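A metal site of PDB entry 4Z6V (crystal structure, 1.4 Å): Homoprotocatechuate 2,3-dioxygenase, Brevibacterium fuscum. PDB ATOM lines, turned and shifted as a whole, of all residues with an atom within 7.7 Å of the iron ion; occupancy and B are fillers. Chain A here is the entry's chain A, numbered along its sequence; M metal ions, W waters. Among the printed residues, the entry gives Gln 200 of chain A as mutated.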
ATOM      1  N   ASP A 154      11.535 -25.521  -7.517  1.00  0.00           N
ATOM      2  CA  ASP A 154      12.530 -25.466  -6.451  1.00  0.00           C
ATOM      3  C   ASP A 154      12.640 -24.145  -5.680  1.00  0.00           C
ATOM      4  O   ASP A 154      12.696 -24.157  -4.437  1.00  0.00           O
ATOM      5  CB  ASP A 154      13.928 -25.881  -6.918  1.00  0.00           C
ATOM      6  CG  ASP A 154      14.845 -26.130  -5.740  1.00  0.00           C
ATOM      7  OD1 ASP A 154      14.666 -27.165  -5.073  1.00  0.00           O
ATOM      8  OD2 ASP A 154      15.675 -25.242  -5.429  1.00  0.00           O
ATOM      9  N   HIS A 155      12.726 -23.042  -6.405  1.00  0.00           N
ATOM     10  CA  HIS A 155      12.956 -21.748  -5.759  1.00  0.00           C
ATOM     11  C   HIS A 155      12.687 -20.571  -6.664  1.00  0.00           C
ATOM     12  O   HIS A 155      12.559 -20.683  -7.869  1.00  0.00           O
ATOM     13  CB  HIS A 155      14.402 -21.673  -5.195  1.00  0.00           C
ATOM     14  CG  HIS A 155      15.495 -21.668  -6.222  1.00  0.00           C
ATOM     15  ND1 HIS A 155      16.122 -22.823  -6.615  1.00  0.00           N
ATOM     16  CD2 HIS A 155      16.122 -20.661  -6.867  1.00  0.00           C
ATOM     17  CE1 HIS A 155      17.084 -22.534  -7.480  1.00  0.00           C
ATOM     18  NE2 HIS A 155      17.120 -21.227  -7.627  1.00  0.00           N
ATOM     19  N   PHE A 156      12.686 -19.407  -6.020  1.00  0.00           N
ATOM     20  CA  PHE A 156      12.729 -18.112  -6.667  1.00  0.00           C
ATOM     21  C   PHE A 156      14.070 -17.445  -6.351  1.00  0.00           C
ATOM     22  O   PHE A 156      14.740 -17.792  -5.352  1.00  0.00           O
ATOM     23  CB  PHE A 156      11.631 -17.175  -6.110  1.00  0.00           C
ATOM     24  CG  PHE A 156      10.242 -17.795  -6.016  1.00  0.00           C
ATOM     25  CD1 PHE A 156       9.615 -18.361  -7.119  1.00  0.00           C
ATOM     26  CD2 PHE A 156       9.569 -17.798  -4.796  1.00  0.00           C
ATOM     27  CE1 PHE A 156       8.341 -18.885  -7.014  1.00  0.00           C
ATOM     28  CE2 PHE A 156       8.300 -18.319  -4.678  1.00  0.00           C
ATOM     29  CZ  PHE A 156       7.691 -18.861  -5.786  1.00  0.00           C
ATOM     30  N   ASN A 157      14.429 -16.467  -7.163  1.00  0.00           N
ATOM     31  CA  ASN A 157      15.606 -15.632  -6.868  1.00  0.00           C
ATOM     32  C   ASN A 157      15.242 -14.179  -7.212  1.00  0.00           C
ATOM     33  O   ASN A 157      14.814 -13.865  -8.331  1.00  0.00           O
ATOM     34  CB  ASN A 157      16.810 -16.147  -7.656  1.00  0.00           C
ATOM     35  CG  ASN A 157      18.106 -15.435  -7.304  1.00  0.00           C
ATOM     36  OD1 ASN A 157      18.179 -14.226  -7.371  1.00  0.00           O
ATOM     37  ND2 ASN A 157      19.126 -16.192  -6.907  1.00  0.00           N
ATOM     38  N   TRP A 192      21.207 -17.035   0.140  1.00  0.00           N
ATOM     39  CA  TRP A 192      20.265 -18.102  -0.191  1.00  0.00           C
ATOM     40  C   TRP A 192      19.609 -18.547   1.092  1.00  0.00           C
ATOM     41  O   TRP A 192      20.295 -18.673   2.106  1.00  0.00           O
ATOM     42  CB  TRP A 192      21.027 -19.279  -0.811  1.00  0.00           C
ATOM     43  CG  TRP A 192      21.496 -19.070  -2.229  1.00  0.00           C
ATOM     44  CD1 TRP A 192      20.917 -19.586  -3.346  1.00  0.00           C
ATOM     45  CD2 TRP A 192      22.624 -18.290  -2.691  1.00  0.00           C
ATOM     46  NE1 TRP A 192      21.603 -19.203  -4.468  1.00  0.00           N
ATOM     47  CE2 TRP A 192      22.646 -18.388  -4.096  1.00  0.00           C
ATOM     48  CE3 TRP A 192      23.601 -17.528  -2.055  1.00  0.00           C
ATOM     49  CZ2 TRP A 192      23.622 -17.782  -4.883  1.00  0.00           C
ATOM     50  CZ3 TRP A 192      24.572 -16.911  -2.833  1.00  0.00           C
ATOM     51  CH2 TRP A 192      24.565 -17.026  -4.238  1.00  0.00           C
ATOM     52  N   GLN A 200      17.385 -23.609  -0.824  1.00  0.00           N
ATOM     53  CA  GLN A 200      16.656 -22.364  -1.027  1.00  0.00           C
ATOM     54  C   GLN A 200      15.197 -22.584  -1.349  1.00  0.00           C
ATOM     55  O   GLN A 200      14.835 -23.533  -2.069  1.00  0.00           O
ATOM     56  CB  GLN A 200      17.331 -21.520  -2.124  1.00  0.00           C
ATOM     57  CG  GLN A 200      17.566 -22.341  -3.399  1.00  0.00           C
ATOM     58  CD  GLN A 200      18.375 -21.607  -4.433  1.00  0.00           C
ATOM     59  OE1 GLN A 200      18.202 -20.390  -4.637  1.00  0.00           O
ATOM     60  NE2 GLN A 200      19.287 -22.324  -5.074  1.00  0.00           N
ATOM     61  N   ALA A 203      15.958 -16.516  -2.711  1.00  0.00           N
ATOM     62  CA  ALA A 203      17.354 -16.119  -2.682  1.00  0.00           C
ATOM     63  C   ALA A 203      17.435 -14.651  -3.080  1.00  0.00           C
ATOM     64  O   ALA A 203      16.548 -14.136  -3.756  1.00  0.00           O
ATOM     65  CB  ALA A 203      18.200 -16.997  -3.594  1.00  0.00           C
ATOM     66  N   THR A 205      19.841 -11.706  -4.815  1.00  0.00           N
ATOM     67  CA  THR A 205      20.984 -11.327  -5.665  1.00  0.00           C
ATOM     68  C   THR A 205      21.081  -9.813  -5.586  1.00  0.00           C
ATOM     69  O   THR A 205      20.108  -9.127  -5.857  1.00  0.00           O
ATOM     70  CB  THR A 205      20.761 -11.788  -7.118  1.00  0.00           C
ATOM     71  OG1 THR A 205      20.636 -13.221  -7.144  1.00  0.00           O
ATOM     72  CG2 THR A 205      21.904 -11.352  -8.033  1.00  0.00           C
ATOM     73  N   HIS A 213      14.910 -12.312 -10.491  1.00  0.00           N
ATOM     74  CA  HIS A 213      16.026 -12.841 -11.238  1.00  0.00           C
ATOM     75  C   HIS A 213      15.635 -14.100 -12.031  1.00  0.00           C
ATOM     76  O   HIS A 213      15.893 -14.172 -13.238  1.00  0.00           O
ATOM     77  CB  HIS A 213      17.253 -13.133 -10.358  1.00  0.00           C
ATOM     78  CG  HIS A 213      18.498 -13.241 -11.165  1.00  0.00           C
ATOM     79  ND1 HIS A 213      18.835 -14.398 -11.831  1.00  0.00           N
ATOM     80  CD2 HIS A 213      19.454 -12.341 -11.481  1.00  0.00           C
ATOM     81  CE1 HIS A 213      19.954 -14.213 -12.495  1.00  0.00           C
ATOM     82  NE2 HIS A 213      20.351 -12.975 -12.310  1.00  0.00           N
ATOM     83  N   HIS A 214      15.058 -15.082 -11.334  1.00  0.00           N
ATOM     84  CA  HIS A 214      14.600 -16.303 -12.004  1.00  0.00           C
ATOM     85  C   HIS A 214      13.606 -17.081 -11.147  1.00  0.00           C
ATOM     86  O   HIS A 214      13.492 -16.855  -9.929  1.00  0.00           O
ATOM     87  CB  HIS A 214      15.797 -17.209 -12.438  1.00  0.00           C
ATOM     88  CG  HIS A 214      16.715 -17.637 -11.322  1.00  0.00           C
ATOM     89  ND1 HIS A 214      17.850 -16.941 -11.000  1.00  0.00           N
ATOM     90  CD2 HIS A 214      16.675 -18.699 -10.483  1.00  0.00           C
ATOM     91  CE1 HIS A 214      18.495 -17.551 -10.030  1.00  0.00           C
ATOM     92  NE2 HIS A 214      17.801 -18.620  -9.688  1.00  0.00           N
ATOM     93  N   VAL A 215      12.937 -18.028 -11.814  1.00  0.00           N
ATOM     94  CA  VAL A 215      12.226 -19.126 -11.178  1.00  0.00           C
ATOM     95  C   VAL A 215      12.969 -20.407 -11.537  1.00  0.00           C
ATOM     96  O   VAL A 215      13.401 -20.561 -12.687  1.00  0.00           O
ATOM     97  CB  VAL A 215      10.755 -19.168 -11.667  1.00  0.00           C
ATOM     98  CG1 VAL A 215       9.991 -20.328 -11.029  1.00  0.00           C
ATOM     99  CG2 VAL A 215      10.053 -17.833 -11.368  1.00  0.00           C
ATOM    100  N   ALA A 216      13.131 -21.314 -10.579  1.00  0.00           N
ATOM    101  CA  ALA A 216      13.884 -22.540 -10.795  1.00  0.00           C
ATOM    102  C   ALA A 216      13.020 -23.771 -10.624  1.00  0.00           C
ATOM    103  O   ALA A 216      12.286 -23.908  -9.619  1.00  0.00           O
ATOM    104  CB  ALA A 216      15.057 -22.631  -9.842  1.00  0.00           C
ATOM    105  N   HIS A 248      27.041 -25.563  -9.853  1.00  0.00           N
ATOM    106  CA  HIS A 248      27.185 -24.401  -8.982  1.00  0.00           C
ATOM    107  C   HIS A 248      28.213 -24.673  -7.879  1.00  0.00           C
ATOM    108  O   HIS A 248      28.364 -25.813  -7.437  1.00  0.00           O
ATOM    109  CB  HIS A 248      25.878 -24.077  -8.264  1.00  0.00           C
ATOM    110  CG  HIS A 248      24.872 -23.357  -9.105  1.00  0.00           C
ATOM    111  ND1 HIS A 248      25.147 -22.190  -9.791  1.00  0.00           N
ATOM    112  CD2 HIS A 248      23.548 -23.597  -9.279  1.00  0.00           C
ATOM    113  CE1 HIS A 248      24.045 -21.764 -10.366  1.00  0.00           C
ATOM    114  NE2 HIS A 248      23.055 -22.590 -10.065  1.00  0.00           N
ATOM    115  N   VAL A 250      28.016 -22.380  -4.877  1.00  0.00           N
ATOM    116  CA  VAL A 250      26.895 -22.156  -3.980  1.00  0.00           C
ATOM    117  C   VAL A 250      25.735 -23.082  -4.407  1.00  0.00           C
ATOM    118  O   VAL A 250      25.321 -23.025  -5.573  1.00  0.00           O
ATOM    119  CB  VAL A 250      26.387 -20.710  -4.058  1.00  0.00           C
ATOM    120  CG1 VAL A 250      25.107 -20.570  -3.264  1.00  0.00           C
ATOM    121  CG2 VAL A 250      27.429 -19.728  -3.527  1.00  0.00           C
ATOM    122  N   SER A 251      25.264 -23.887  -3.467  1.00  0.00           N
ATOM    123  CA  SER A 251      24.207 -24.900  -3.619  1.00  0.00           C
ATOM    124  C   SER A 251      24.683 -26.265  -4.057  1.00  0.00           C
ATOM    125  O   SER A 251      23.979 -27.253  -3.827  1.00  0.00           O
ATOM    126  CB  SER A 251      23.040 -24.452  -4.498  1.00  0.00           C
ATOM    127  OG  SER A 251      23.321 -24.649  -5.888  1.00  0.00           O
ATOM    128  N   TYR A 255      23.052 -27.166 -13.018  1.00  0.00           N
ATOM    129  CA  TYR A 255      22.178 -26.056 -13.362  1.00  0.00           C
ATOM    130  C   TYR A 255      22.237 -25.660 -14.831  1.00  0.00           C
ATOM    131  O   TYR A 255      23.203 -25.964 -15.561  1.00  0.00           O
ATOM    132  CB  TYR A 255      22.525 -24.831 -12.489  1.00  0.00           C
ATOM    133  CG  TYR A 255      23.786 -24.115 -12.942  1.00  0.00           C
ATOM    134  CD1 TYR A 255      23.744 -23.142 -13.909  1.00  0.00           C
ATOM    135  CD2 TYR A 255      25.004 -24.416 -12.377  1.00  0.00           C
ATOM    136  CE1 TYR A 255      24.910 -22.485 -14.334  1.00  0.00           C
ATOM    137  CE2 TYR A 255      26.178 -23.754 -12.768  1.00  0.00           C
ATOM    138  CZ  TYR A 255      26.134 -22.815 -13.766  1.00  0.00           C
ATOM    139  OH  TYR A 255      27.256 -22.135 -14.177  1.00  0.00           O
ATOM    140  N   TYR A 257      20.570 -21.977 -17.147  1.00  0.00           N
ATOM    141  CA  TYR A 257      19.681 -20.811 -17.283  1.00  0.00           C
ATOM    142  C   TYR A 257      19.285 -20.579 -18.722  1.00  0.00           C
ATOM    143  O   TYR A 257      20.135 -20.460 -19.618  1.00  0.00           O
ATOM    144  CB  TYR A 257      20.342 -19.549 -16.739  1.00  0.00           C
ATOM    145  CG  TYR A 257      20.760 -19.611 -15.293  1.00  0.00           C
ATOM    146  CD1 TYR A 257      19.871 -19.327 -14.265  1.00  0.00           C
ATOM    147  CD2 TYR A 257      22.059 -19.996 -14.943  1.00  0.00           C
ATOM    148  CE1 TYR A 257      20.242 -19.401 -12.945  1.00  0.00           C
ATOM    149  CE2 TYR A 257      22.434 -20.067 -13.610  1.00  0.00           C
ATOM    150  CZ  TYR A 257      21.540 -19.766 -12.605  1.00  0.00           C
ATOM    151  OH  TYR A 257      21.961 -19.882 -11.308  1.00  0.00           O
ATOM    152  N   GLU A 267      15.712 -21.159 -14.367  1.00  0.00           N
ATOM    153  CA  GLU A 267      16.806 -22.058 -14.016  1.00  0.00           C
ATOM    154  C   GLU A 267      16.263 -23.469 -13.967  1.00  0.00           C
ATOM    155  O   GLU A 267      15.177 -23.731 -13.428  1.00  0.00           O
ATOM    156  CB  GLU A 267      17.418 -21.659 -12.682  1.00  0.00           C
ATOM    157  CG  GLU A 267      18.672 -22.443 -12.334  1.00  0.00           C
ATOM    158  CD  GLU A 267      19.242 -22.104 -10.994  1.00  0.00           C
ATOM    159  OE1 GLU A 267      18.612 -21.312 -10.278  1.00  0.00           O
ATOM    160  OE2 GLU A 267      20.316 -22.668 -10.632  1.00  0.00           O
ATOM    161  N   ILE A 268      17.074 -24.390 -14.474  1.00  0.00           N
ATOM    162  CA  ILE A 268      16.853 -25.812 -14.258  1.00  0.00           C
ATOM    163  C   ILE A 268      17.963 -26.288 -13.326  1.00  0.00           C
ATOM    164  O   ILE A 268      19.098 -25.848 -13.473  1.00  0.00           O
ATOM    165  CB  ILE A 268      16.874 -26.621 -15.583  1.00  0.00           C
ATOM    166  CG1 ILE A 268      16.226 -25.867 -16.779  1.00  0.00           C
ATOM    167  CG2 ILE A 268      16.183 -27.956 -15.366  1.00  0.00           C
ATOM    168  CD1 ILE A 268      14.786 -25.508 -16.627  1.00  0.00           C
ATOM    169  N   TYR A 269      17.635 -27.167 -12.396  1.00  0.00           N
ATOM    170  CA  TYR A 269      18.421 -27.337 -11.183  1.00  0.00           C
ATOM    171  C   TYR A 269      18.279 -28.768 -10.680  1.00  0.00           C
ATOM    172  O   TYR A 269      17.189 -29.327 -10.718  1.00  0.00           O
ATOM    173  CB  TYR A 269      17.866 -26.370 -10.171  1.00  0.00           C
ATOM    174  CG  TYR A 269      18.467 -26.215  -8.796  1.00  0.00           C
ATOM    175  CD1 TYR A 269      19.393 -25.209  -8.524  1.00  0.00           C
ATOM    176  CD2 TYR A 269      17.995 -26.958  -7.718  1.00  0.00           C
ATOM    177  CE1 TYR A 269      19.839 -24.993  -7.241  1.00  0.00           C
ATOM    178  CE2 TYR A 269      18.437 -26.742  -6.426  1.00  0.00           C
ATOM    179  CZ  TYR A 269      19.381 -25.755  -6.190  1.00  0.00           C
ATOM    180  OH  TYR A 269      19.825 -25.468  -4.918  1.00  0.00           O
ATOM    181  N   ARG A 293      30.239 -19.565  -8.352  1.00  0.00           N
ATOM    182  CA  ARG A 293      28.978 -19.566  -9.103  1.00  0.00           C
ATOM    183  C   ARG A 293      28.943 -20.716 -10.093  1.00  0.00           C
ATOM    184  O   ARG A 293      27.985 -21.485 -10.143  1.00  0.00           O
ATOM    185  CB  ARG A 293      28.721 -18.225  -9.801  1.00  0.00           C
ATOM    186  CG  ARG A 293      28.334 -17.123  -8.823  1.00  0.00           C
ATOM    187  CD  ARG A 293      27.594 -15.969  -9.458  1.00  0.00           C
ATOM    188  NE  ARG A 293      27.107 -15.011  -8.474  1.00  0.00           N
ATOM    189  CZ  ARG A 293      25.943 -15.074  -7.827  1.00  0.00           C
ATOM    190  NH1 ARG A 293      25.113 -16.110  -7.955  1.00  0.00           N
ATOM    191  NH2 ARG A 293      25.619 -14.095  -6.995  1.00  0.00           N
ATOM    192  N   TRP A 304      23.702 -12.077 -17.062  1.00  0.00           N
ATOM    193  CA  TRP A 304      23.215 -12.783 -15.883  1.00  0.00           C
ATOM    194  C   TRP A 304      23.155 -11.830 -14.693  1.00  0.00           C
ATOM    195  O   TRP A 304      22.264 -11.919 -13.823  1.00  0.00           O
ATOM    196  CB  TRP A 304      24.091 -14.019 -15.581  1.00  0.00           C
ATOM    197  CG  TRP A 304      23.416 -14.990 -14.633  1.00  0.00           C
ATOM    198  CD1 TRP A 304      22.585 -16.035 -14.986  1.00  0.00           C
ATOM    199  CD2 TRP A 304      23.465 -14.988 -13.211  1.00  0.00           C
ATOM    200  NE1 TRP A 304      22.124 -16.668 -13.862  1.00  0.00           N
ATOM    201  CE2 TRP A 304      22.649 -16.051 -12.755  1.00  0.00           C
ATOM    202  CE3 TRP A 304      24.102 -14.167 -12.266  1.00  0.00           C
ATOM    203  CZ2 TRP A 304      22.465 -16.320 -11.410  1.00  0.00           C
ATOM    204  CZ3 TRP A 304      23.910 -14.428 -10.935  1.00  0.00           C
ATOM    205  CH2 TRP A 304      23.105 -15.492 -10.507  1.00  0.00           C
HETATM  206 FE    FE M   1      18.856 -20.174  -8.533  1.00  0.00          FE
HETATM  207  O   HOH W   1      20.226 -21.750  -7.900  1.00  0.00           O
HETATM  208  O   HOH W   2      19.105 -19.052  -6.733  1.00  0.00           O
HETATM  209  O   HOH W   3      20.809 -19.251  -9.205  1.00  0.00           O
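The side-chain hydroxyl (OH) of Tyr 257 sits at hydrogen-bond distance from the side-chain carboxylate (OE2) of Glu 267, at 3.3 Å. A ring nitrogen (NE2) of His 248 is in hydrogen-bond range of the side-chain carboxylate of Glu 267, 2.8 Å away. The backbone NH of Glu 267 is in hydrogen-bond range of the backbone carbonyl oxygen of Val 215 (2.9 Å). O of His 214 is in hydrogen-bond range of N of Asn 157 (2.9 Å). NE2 of His 155 sits close to OE1 of Gln 200, 3.3 Å away. The backbone NH (N) of Ala 216 lies within hydrogen-bond range of the backbone carbonyl oxygen (O) of His 155. ND1 of His 155 is in hydrogen-bond range of OD2 of Asp 154 (2.7 Å). The side-chain amide nitrogen (NE2) of Gln 200 is in hydrogen-bond range of the side-chain hydroxyl (OH) of Tyr 269 (3.2 Å).
Residues that only touch the iron ion: Gln 200. Four residues have an atom within 4 Å of the iron ion: His 155, Gln 200, His 214 and Glu 267. The nearest printed residue that does not touch the iron ion is Tyr 257 (4.2 Å).
The iron ion is bound by OE1 of Glu 267 (2.1 Å), water W2 (2.1 Å), water W1 (2.2 Å), NE2 of His 214 (2.2 Å), NE2 of His 155 (2.2 Å) and water W3 (2.3 Å).
Water W2 lies within hydrogen-bond range of OE1 of Gln 200 (2.6 Å), ND2 of Asn 157 (2.9 Å) and NE1 of Trp 192 (3.4 Å). Water W1 bridges OE2 of Glu 267 (2.9 Å) and NE2 of Gln 200 (3.0 Å).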
